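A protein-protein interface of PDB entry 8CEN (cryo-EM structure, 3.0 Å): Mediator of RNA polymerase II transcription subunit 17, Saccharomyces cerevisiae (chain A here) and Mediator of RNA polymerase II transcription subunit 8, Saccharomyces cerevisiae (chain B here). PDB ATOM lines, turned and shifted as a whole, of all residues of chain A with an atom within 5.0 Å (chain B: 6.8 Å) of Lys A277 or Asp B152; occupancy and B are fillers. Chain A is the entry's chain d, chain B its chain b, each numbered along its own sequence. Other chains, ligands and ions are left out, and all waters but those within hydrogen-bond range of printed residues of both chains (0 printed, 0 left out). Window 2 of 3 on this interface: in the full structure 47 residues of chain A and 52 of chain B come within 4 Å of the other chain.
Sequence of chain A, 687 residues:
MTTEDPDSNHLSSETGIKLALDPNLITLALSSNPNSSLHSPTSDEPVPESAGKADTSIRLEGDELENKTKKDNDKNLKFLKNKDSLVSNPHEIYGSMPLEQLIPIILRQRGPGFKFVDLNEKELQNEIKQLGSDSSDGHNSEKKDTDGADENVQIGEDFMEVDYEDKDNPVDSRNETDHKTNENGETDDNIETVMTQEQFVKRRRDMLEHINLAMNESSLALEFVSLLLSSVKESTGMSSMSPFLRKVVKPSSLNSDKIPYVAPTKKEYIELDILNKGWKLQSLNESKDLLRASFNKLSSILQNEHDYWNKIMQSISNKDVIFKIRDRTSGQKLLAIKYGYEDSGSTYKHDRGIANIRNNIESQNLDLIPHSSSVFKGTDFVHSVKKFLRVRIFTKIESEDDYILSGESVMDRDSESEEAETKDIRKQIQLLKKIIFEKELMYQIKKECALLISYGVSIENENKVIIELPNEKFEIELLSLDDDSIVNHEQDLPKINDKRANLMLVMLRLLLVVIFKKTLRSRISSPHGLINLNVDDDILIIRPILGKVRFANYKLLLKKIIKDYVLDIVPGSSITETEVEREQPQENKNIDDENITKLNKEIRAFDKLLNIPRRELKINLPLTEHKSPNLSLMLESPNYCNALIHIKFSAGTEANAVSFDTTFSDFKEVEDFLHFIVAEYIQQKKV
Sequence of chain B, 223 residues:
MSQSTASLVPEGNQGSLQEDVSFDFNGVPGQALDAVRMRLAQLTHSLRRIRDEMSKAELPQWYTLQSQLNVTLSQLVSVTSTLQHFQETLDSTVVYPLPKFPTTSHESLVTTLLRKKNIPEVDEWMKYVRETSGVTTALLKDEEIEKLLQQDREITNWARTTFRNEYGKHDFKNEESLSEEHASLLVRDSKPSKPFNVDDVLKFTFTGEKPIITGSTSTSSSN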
ATOM      1  N   ASP A 273       3.988 -17.078 -18.787  1.00  0.00           N
ATOM      2  CA  ASP A 273       4.730 -16.924 -17.540  1.00  0.00           C
ATOM      3  C   ASP A 273       5.077 -18.274 -16.922  1.00  0.00           C
ATOM      4  O   ASP A 273       6.198 -18.469 -16.441  1.00  0.00           O
ATOM      5  CB  ASP A 273       3.916 -16.076 -16.564  1.00  0.00           C
ATOM      6  CG  ASP A 273       4.138 -14.588 -16.762  1.00  0.00           C
ATOM      7  OD1 ASP A 273       4.844 -14.211 -17.720  1.00  0.00           O
ATOM      8  OD2 ASP A 273       3.605 -13.793 -15.958  1.00  0.00           O
ATOM      9  N   ILE A 274       4.133 -19.222 -16.922  1.00  0.00           N
ATOM     10  CA  ILE A 274       4.413 -20.534 -16.348  1.00  0.00           C
ATOM     11  C   ILE A 274       5.372 -21.311 -17.247  1.00  0.00           C
ATOM     12  O   ILE A 274       6.220 -22.073 -16.755  1.00  0.00           O
ATOM     13  CB  ILE A 274       3.088 -21.283 -16.066  1.00  0.00           C
ATOM     14  CG1 ILE A 274       3.309 -22.511 -15.195  1.00  0.00           C
ATOM     15  CG2 ILE A 274       2.374 -21.728 -17.327  1.00  0.00           C
ATOM     16  CD1 ILE A 274       2.005 -23.046 -14.658  1.00  0.00           C
ATOM     17  N   LEU A 275       5.295 -21.087 -18.567  1.00  0.00           N
ATOM     18  CA  LEU A 275       6.295 -21.617 -19.489  1.00  0.00           C
ATOM     19  C   LEU A 275       7.681 -21.068 -19.180  1.00  0.00           C
ATOM     20  O   LEU A 275       8.667 -21.818 -19.163  1.00  0.00           O
ATOM     21  CB  LEU A 275       5.894 -21.262 -20.918  1.00  0.00           C
ATOM     22  CG  LEU A 275       6.879 -21.478 -22.062  1.00  0.00           C
ATOM     23  CD1 LEU A 275       7.221 -22.947 -22.228  1.00  0.00           C
ATOM     24  CD2 LEU A 275       6.301 -20.884 -23.336  1.00  0.00           C
ATOM     25  N   ASN A 276       7.767 -19.759 -18.929  1.00  0.00           N
ATOM     26  CA  ASN A 276       9.035 -19.128 -18.584  1.00  0.00           C
ATOM     27  C   ASN A 276       9.591 -19.686 -17.283  1.00  0.00           C
ATOM     28  O   ASN A 276      10.789 -19.970 -17.190  1.00  0.00           O
ATOM     29  CB  ASN A 276       8.845 -17.615 -18.480  1.00  0.00           C
ATOM     30  CG  ASN A 276      10.156 -16.864 -18.364  1.00  0.00           C
ATOM     31  OD1 ASN A 276      11.230 -17.421 -18.585  1.00  0.00           O
ATOM     32  ND2 ASN A 276      10.071 -15.586 -18.018  1.00  0.00           N
ATOM     33  N   LYS A 277       8.729 -19.864 -16.279  1.00  0.00           N
ATOM     34  CA  LYS A 277       9.166 -20.396 -14.990  1.00  0.00           C
ATOM     35  C   LYS A 277       9.719 -21.809 -15.133  1.00  0.00           C
ATOM     36  O   LYS A 277      10.819 -22.109 -14.649  1.00  0.00           O
ATOM     37  CB  LYS A 277       8.000 -20.370 -14.000  1.00  0.00           C
ATOM     38  CG  LYS A 277       8.267 -21.106 -12.698  1.00  0.00           C
ATOM     39  CD  LYS A 277       7.187 -20.811 -11.670  1.00  0.00           C
ATOM     40  CE  LYS A 277       7.403 -21.607 -10.396  1.00  0.00           C
ATOM     41  NZ  LYS A 277       7.218 -23.068 -10.609  1.00  0.00           N
ATOM     42  N   GLY A 278       8.988 -22.678 -15.835  1.00  0.00           N
ATOM     43  CA  GLY A 278       9.458 -24.043 -16.019  1.00  0.00           C
ATOM     44  C   GLY A 278      10.724 -24.134 -16.848  1.00  0.00           C
ATOM     45  O   GLY A 278      11.614 -24.940 -16.552  1.00  0.00           O
ATOM     46  N   TRP A 279      10.843 -23.297 -17.879  1.00  0.00           N
ATOM     47  CA  TRP A 279      11.990 -23.425 -18.764  1.00  0.00           C
ATOM     48  C   TRP A 279      13.231 -22.830 -18.097  1.00  0.00           C
ATOM     49  O   TRP A 279      14.338 -23.362 -18.248  1.00  0.00           O
ATOM     50  CB  TRP A 279      11.665 -22.759 -20.106  1.00  0.00           C
ATOM     51  CG  TRP A 279      12.590 -23.081 -21.254  1.00  0.00           C
ATOM     52  CD1 TRP A 279      13.897 -23.459 -21.196  1.00  0.00           C
ATOM     53  CD2 TRP A 279      12.232 -23.113 -22.639  1.00  0.00           C
ATOM     54  NE1 TRP A 279      14.384 -23.694 -22.456  1.00  0.00           N
ATOM     55  CE2 TRP A 279      13.378 -23.491 -23.361  1.00  0.00           C
ATOM     56  CE3 TRP A 279      11.053 -22.847 -23.337  1.00  0.00           C
ATOM     57  CZ2 TRP A 279      13.381 -23.606 -24.745  1.00  0.00           C
ATOM     58  CZ3 TRP A 279      11.060 -22.958 -24.708  1.00  0.00           C
ATOM     59  CH2 TRP A 279      12.211 -23.346 -25.397  1.00  0.00           C
ATOM     60  N   LYS A 280      13.057 -21.755 -17.317  1.00  0.00           N
ATOM     61  CA  LYS A 280      14.154 -21.235 -16.505  1.00  0.00           C
ATOM     62  C   LYS A 280      14.589 -22.246 -15.451  1.00  0.00           C
ATOM     63  O   LYS A 280      15.782 -22.363 -15.155  1.00  0.00           O
ATOM     64  CB  LYS A 280      13.750 -19.918 -15.841  1.00  0.00           C
ATOM     65  CG  LYS A 280      13.690 -18.705 -16.760  1.00  0.00           C
ATOM     66  CD  LYS A 280      14.969 -18.517 -17.549  1.00  0.00           C
ATOM     67  CE  LYS A 280      14.797 -17.453 -18.619  1.00  0.00           C
ATOM     68  NZ  LYS A 280      14.049 -16.270 -18.108  1.00  0.00           N
ATOM     69  N   LEU A 281      13.635 -22.985 -14.872  1.00  0.00           N
ATOM     70  CA  LEU A 281      13.994 -24.049 -13.936  1.00  0.00           C
ATOM     71  C   LEU A 281      14.796 -25.153 -14.618  1.00  0.00           C
ATOM     72  O   LEU A 281      15.758 -25.679 -14.042  1.00  0.00           O
ATOM     73  CB  LEU A 281      12.735 -24.623 -13.290  1.00  0.00           C
ATOM     74  CG  LEU A 281      12.287 -23.933 -12.004  1.00  0.00           C
ATOM     75  CD1 LEU A 281      10.866 -24.328 -11.642  1.00  0.00           C
ATOM     76  CD2 LEU A 281      13.247 -24.294 -10.887  1.00  0.00           C
ATOM     77  N   VAL B 129       9.238 -29.172 -20.334  1.00  0.00           N
ATOM     78  CA  VAL B 129       9.551 -28.181 -19.305  1.00  0.00           C
ATOM     79  C   VAL B 129       8.271 -27.650 -18.662  1.00  0.00           C
ATOM     80  O   VAL B 129       8.269 -27.296 -17.476  1.00  0.00           O
ATOM     81  CB  VAL B 129      10.443 -27.049 -19.857  1.00  0.00           C
ATOM     82  CG1 VAL B 129      11.729 -27.621 -20.431  1.00  0.00           C
ATOM     83  CG2 VAL B 129       9.725 -26.205 -20.891  1.00  0.00           C
ATOM     84  N   THR B 132       7.600 -30.350 -16.091  1.00  0.00           N
ATOM     85  CA  THR B 132       8.566 -30.318 -14.997  1.00  0.00           C
ATOM     86  C   THR B 132       8.618 -28.974 -14.280  1.00  0.00           C
ATOM     87  O   THR B 132       9.438 -28.812 -13.370  1.00  0.00           O
ATOM     88  CB  THR B 132       9.969 -30.682 -15.497  1.00  0.00           C
ATOM     89  OG1 THR B 132      10.419 -29.704 -16.441  1.00  0.00           O
ATOM     90  CG2 THR B 132       9.975 -32.067 -16.131  1.00  0.00           C
ATOM     91  N   SER B 133       7.786 -28.007 -14.683  1.00  0.00           N
ATOM     92  CA  SER B 133       7.614 -26.793 -13.889  1.00  0.00           C
ATOM     93  C   SER B 133       7.099 -27.093 -12.483  1.00  0.00           C
ATOM     94  O   SER B 133       7.356 -26.321 -11.552  1.00  0.00           O
ATOM     95  CB  SER B 133       6.654 -25.838 -14.596  1.00  0.00           C
ATOM     96  OG  SER B 133       6.464 -24.656 -13.839  1.00  0.00           O
ATOM     97  N   GLY B 134       6.374 -28.199 -12.308  1.00  0.00           N
ATOM     98  CA  GLY B 134       5.799 -28.556 -11.031  1.00  0.00           C
ATOM     99  C   GLY B 134       4.418 -27.995 -10.786  1.00  0.00           C
ATOM    100  O   GLY B 134       3.761 -28.403  -9.820  1.00  0.00           O
ATOM    101  N   VAL B 135       3.962 -27.075 -11.628  1.00  0.00           N
ATOM    102  CA  VAL B 135       2.623 -26.506 -11.550  1.00  0.00           C
ATOM    103  C   VAL B 135       2.093 -26.363 -12.972  1.00  0.00           C
ATOM    104  O   VAL B 135       2.854 -26.077 -13.904  1.00  0.00           O
ATOM    105  CB  VAL B 135       2.628 -25.170 -10.766  1.00  0.00           C
ATOM    106  CG1 VAL B 135       3.442 -24.097 -11.476  1.00  0.00           C
ATOM    107  CG2 VAL B 135       1.209 -24.685 -10.508  1.00  0.00           C
ATOM    108  N   GLU B 146      -1.921 -16.998 -10.524  1.00  0.00           N
ATOM    109  CA  GLU B 146      -1.450 -15.620 -10.412  1.00  0.00           C
ATOM    110  C   GLU B 146      -0.796 -15.354  -9.061  1.00  0.00           C
ATOM    111  O   GLU B 146       0.254 -14.705  -8.991  1.00  0.00           O
ATOM    112  CB  GLU B 146      -2.606 -14.647 -10.649  1.00  0.00           C
ATOM    113  CG  GLU B 146      -2.979 -14.474 -12.111  1.00  0.00           C
ATOM    114  CD  GLU B 146      -4.108 -13.483 -12.311  1.00  0.00           C
ATOM    115  OE1 GLU B 146      -4.701 -13.046 -11.304  1.00  0.00           O
ATOM    116  OE2 GLU B 146      -4.400 -13.141 -13.476  1.00  0.00           O
ATOM    117  N   LYS B 147      -1.384 -15.864  -7.973  1.00  0.00           N
ATOM    118  CA  LYS B 147      -0.769 -15.642  -6.666  1.00  0.00           C
ATOM    119  C   LYS B 147       0.497 -16.476  -6.491  1.00  0.00           C
ATOM    120  O   LYS B 147       1.430 -16.044  -5.800  1.00  0.00           O
ATOM    121  CB  LYS B 147      -1.782 -15.904  -5.543  1.00  0.00           C
ATOM    122  CG  LYS B 147      -2.233 -17.345  -5.347  1.00  0.00           C
ATOM    123  CD  LYS B 147      -1.527 -18.010  -4.170  1.00  0.00           C
ATOM    124  CE  LYS B 147      -2.092 -19.393  -3.897  1.00  0.00           C
ATOM    125  NZ  LYS B 147      -1.415 -20.053  -2.747  1.00  0.00           N
ATOM    126  N   LEU B 148       0.566 -17.654  -7.124  1.00  0.00           N
ATOM    127  CA  LEU B 148       1.797 -18.437  -7.107  1.00  0.00           C
ATOM    128  C   LEU B 148       2.910 -17.716  -7.858  1.00  0.00           C
ATOM    129  O   LEU B 148       4.059 -17.696  -7.406  1.00  0.00           O
ATOM    130  CB  LEU B 148       1.533 -19.829  -7.691  1.00  0.00           C
ATOM    131  CG  LEU B 148       2.575 -20.956  -7.631  1.00  0.00           C
ATOM    132  CD1 LEU B 148       1.859 -22.294  -7.612  1.00  0.00           C
ATOM    133  CD2 LEU B 148       3.552 -20.931  -8.802  1.00  0.00           C
ATOM    134  N   LEU B 149       2.588 -17.102  -8.997  1.00  0.00           N
ATOM    135  CA  LEU B 149       3.590 -16.316  -9.713  1.00  0.00           C
ATOM    136  C   LEU B 149       3.972 -15.053  -8.950  1.00  0.00           C
ATOM    137  O   LEU B 149       5.124 -14.613  -9.028  1.00  0.00           O
ATOM    138  CB  LEU B 149       3.097 -15.965 -11.118  1.00  0.00           C
ATOM    139  CG  LEU B 149       3.433 -16.925 -12.269  1.00  0.00           C
ATOM    140  CD1 LEU B 149       4.937 -16.962 -12.472  1.00  0.00           C
ATOM    141  CD2 LEU B 149       2.897 -18.336 -12.072  1.00  0.00           C
ATOM    142  N   GLN B 150       3.034 -14.467  -8.201  1.00  0.00           N
ATOM    143  CA  GLN B 150       3.358 -13.296  -7.390  1.00  0.00           C
ATOM    144  C   GLN B 150       4.311 -13.651  -6.253  1.00  0.00           C
ATOM    145  O   GLN B 150       5.297 -12.940  -6.013  1.00  0.00           O
ATOM    146  CB  GLN B 150       2.077 -12.664  -6.846  1.00  0.00           C
ATOM    147  CG  GLN B 150       2.311 -11.467  -5.940  1.00  0.00           C
ATOM    148  CD  GLN B 150       3.119 -10.376  -6.618  1.00  0.00           C
ATOM    149  OE1 GLN B 150       4.305 -10.204  -6.342  1.00  0.00           O
ATOM    150  NE2 GLN B 150       2.478  -9.637  -7.516  1.00  0.00           N
ATOM    151  N   GLN B 151       4.054 -14.755  -5.549  1.00  0.00           N
ATOM    152  CA  GLN B 151       5.003 -15.161  -4.516  1.00  0.00           C
ATOM    153  C   GLN B 151       6.318 -15.638  -5.128  1.00  0.00           C
ATOM    154  O   GLN B 151       7.377 -15.466  -4.518  1.00  0.00           O
ATOM    155  CB  GLN B 151       4.387 -16.224  -3.597  1.00  0.00           C
ATOM    156  CG  GLN B 151       4.118 -17.582  -4.219  1.00  0.00           C
ATOM    157  CD  GLN B 151       5.246 -18.568  -3.987  1.00  0.00           C
ATOM    158  OE1 GLN B 151       5.736 -18.715  -2.867  1.00  0.00           O
ATOM    159  NE2 GLN B 151       5.664 -19.249  -5.047  1.00  0.00           N
ATOM    160  N   ASP B 152       6.278 -16.176  -6.352  1.00  0.00           N
ATOM    161  CA  ASP B 152       7.499 -16.578  -7.043  1.00  0.00           C
ATOM    162  C   ASP B 152       8.378 -15.374  -7.369  1.00  0.00           C
ATOM    163  O   ASP B 152       9.592 -15.393  -7.126  1.00  0.00           O
ATOM    164  CB  ASP B 152       7.133 -17.344  -8.314  1.00  0.00           C
ATOM    165  CG  ASP B 152       8.339 -17.921  -9.017  1.00  0.00           C
ATOM    166  OD1 ASP B 152       8.702 -19.074  -8.706  1.00  0.00           O
ATOM    167  OD2 ASP B 152       8.916 -17.227  -9.881  1.00  0.00           O
ATOM    168  N   ARG B 153       7.778 -14.307  -7.913  1.00  0.00           N
ATOM    169  CA  ARG B 153       8.561 -13.109  -8.204  1.00  0.00           C
ATOM    170  C   ARG B 153       9.001 -12.414  -6.921  1.00  0.00           C
ATOM    171  O   ARG B 153      10.054 -11.766  -6.904  1.00  0.00           O
ATOM    172  CB  ARG B 153       7.784 -12.148  -9.115  1.00  0.00           C
ATOM    173  CG  ARG B 153       6.565 -11.502  -8.488  1.00  0.00           C
ATOM    174  CD  ARG B 153       5.817 -10.562  -9.420  1.00  0.00           C
ATOM    175  NE  ARG B 153       5.227 -11.250 -10.562  1.00  0.00           N
ATOM    176  CZ  ARG B 153       5.670 -11.143 -11.806  1.00  0.00           C
ATOM    177  NH1 ARG B 153       6.687 -10.355 -12.110  1.00  0.00           N
ATOM    178  NH2 ARG B 153       5.070 -11.834 -12.771  1.00  0.00           N
ATOM    179  N   GLU B 154       8.240 -12.571  -5.829  1.00  0.00           N
ATOM    180  CA  GLU B 154       8.707 -12.084  -4.531  1.00  0.00           C
ATOM    181  C   GLU B 154       9.957 -12.832  -4.072  1.00  0.00           C
ATOM    182  O   GLU B 154      10.894 -12.223  -3.538  1.00  0.00           O
ATOM    183  CB  GLU B 154       7.594 -12.210  -3.492  1.00  0.00           C
ATOM    184  CG  GLU B 154       6.554 -11.103  -3.559  1.00  0.00           C
ATOM    185  CD  GLU B 154       7.125  -9.743  -3.214  1.00  0.00           C
ATOM    186  OE1 GLU B 154       7.921  -9.657  -2.255  1.00  0.00           O
ATOM    187  OE2 GLU B 154       6.782  -8.760  -3.902  1.00  0.00           O
ATOM    188  N   ILE B 155       9.987 -14.154  -4.270  1.00  0.00           N
ATOM    189  CA  ILE B 155      11.168 -14.940  -3.908  1.00  0.00           C
ATOM    190  C   ILE B 155      12.370 -14.547  -4.767  1.00  0.00           C
ATOM    191  O   ILE B 155      13.498 -14.435  -4.266  1.00  0.00           O
ATOM    192  CB  ILE B 155      10.862 -16.449  -4.000  1.00  0.00           C
ATOM    193  CG1 ILE B 155       9.780 -16.844  -2.996  1.00  0.00           C
ATOM    194  CG2 ILE B 155      12.091 -17.267  -3.718  1.00  0.00           C
ATOM    195  CD1 ILE B 155       9.241 -18.244  -3.199  1.00  0.00           C
ATOM    196  N   THR B 156      12.148 -14.322  -6.068  1.00  0.00           N
ATOM    197  CA  THR B 156      13.244 -13.868  -6.929  1.00  0.00           C
ATOM    198  C   THR B 156      13.750 -12.488  -6.515  1.00  0.00           C
ATOM    199  O   THR B 156      14.959 -12.222  -6.565  1.00  0.00           O
ATOM    200  CB  THR B 156      12.818 -13.844  -8.398  1.00  0.00           C
ATOM    201  OG1 THR B 156      11.816 -12.841  -8.598  1.00  0.00           O
ATOM    202  CG2 THR B 156      12.307 -15.199  -8.846  1.00  0.00           C
ATOM    203  N   ASN B 157      12.840 -11.595  -6.112  1.00  0.00           N
ATOM    204  CA  ASN B 157      13.245 -10.279  -5.629  1.00  0.00           C
ATOM    205  C   ASN B 157      14.066 -10.388  -4.350  1.00  0.00           C
ATOM    206  O   ASN B 157      15.056  -9.662  -4.174  1.00  0.00           O
ATOM    207  CB  ASN B 157      12.014  -9.404  -5.404  1.00  0.00           C
ATOM    208  CG  ASN B 157      12.322  -7.925  -5.515  1.00  0.00           C
ATOM    209  OD1 ASN B 157      13.483  -7.527  -5.612  1.00  0.00           O
ATOM    210  ND2 ASN B 157      11.281  -7.101  -5.501  1.00  0.00           N
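The backbone carbonyl oxygen (O) of Ser B133 sits at hydrogen-bond distance from the side-chain amino group (NZ) of Lys A277, at 3.4 Å.
Of the printed residues of chain B, Gly A278 touches Val B129 (3.8 Å) and Ser B133 (3.6 Å).
Trp A279 touches none of the printed residues of chain B.
Of the printed residues of chain A, Val B129 touches Gly A278 (3.8 Å).
Printed residues of chain A within 4 Å of Ser B133: Ile A274, Lys A277 and Gly A278.
Of the printed residues of chain A, Val B135 touches Ile A274 (3.2 Å).
Glu B146 touches none of the printed residues of chain A.
The nearest printed residue of chain B that does not touch Lys A277 is Val B135 (4.01 Å).
The nearest printed residue of chain A that does not touch Asp B152 is Leu A281 (6.4 Å).
The nearest printed residue of chain A that does not touch Val B135 is Lys A277 (4.01 Å).
Of the 9 printed residues of chain A, 3 touch a printed residue of chain B.
Hydrophobic or aromatic side chains of chain A that line the printed part of chain B: Ile A274.
Among the printed residues, 6 pairs touch across the chains.
Among the printed residues, merely in contact across the chains: Ile A274 with Val B135, Lys A277 with Asp B152, Gly A278 with Ser B133, Gly A278 with Val B129 and Ile A274 with Ser B133.
The backbone carbonyl oxygen of Val B129 lies close to the side-chain hydroxyl of Thr B132, at 3.4 Å.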
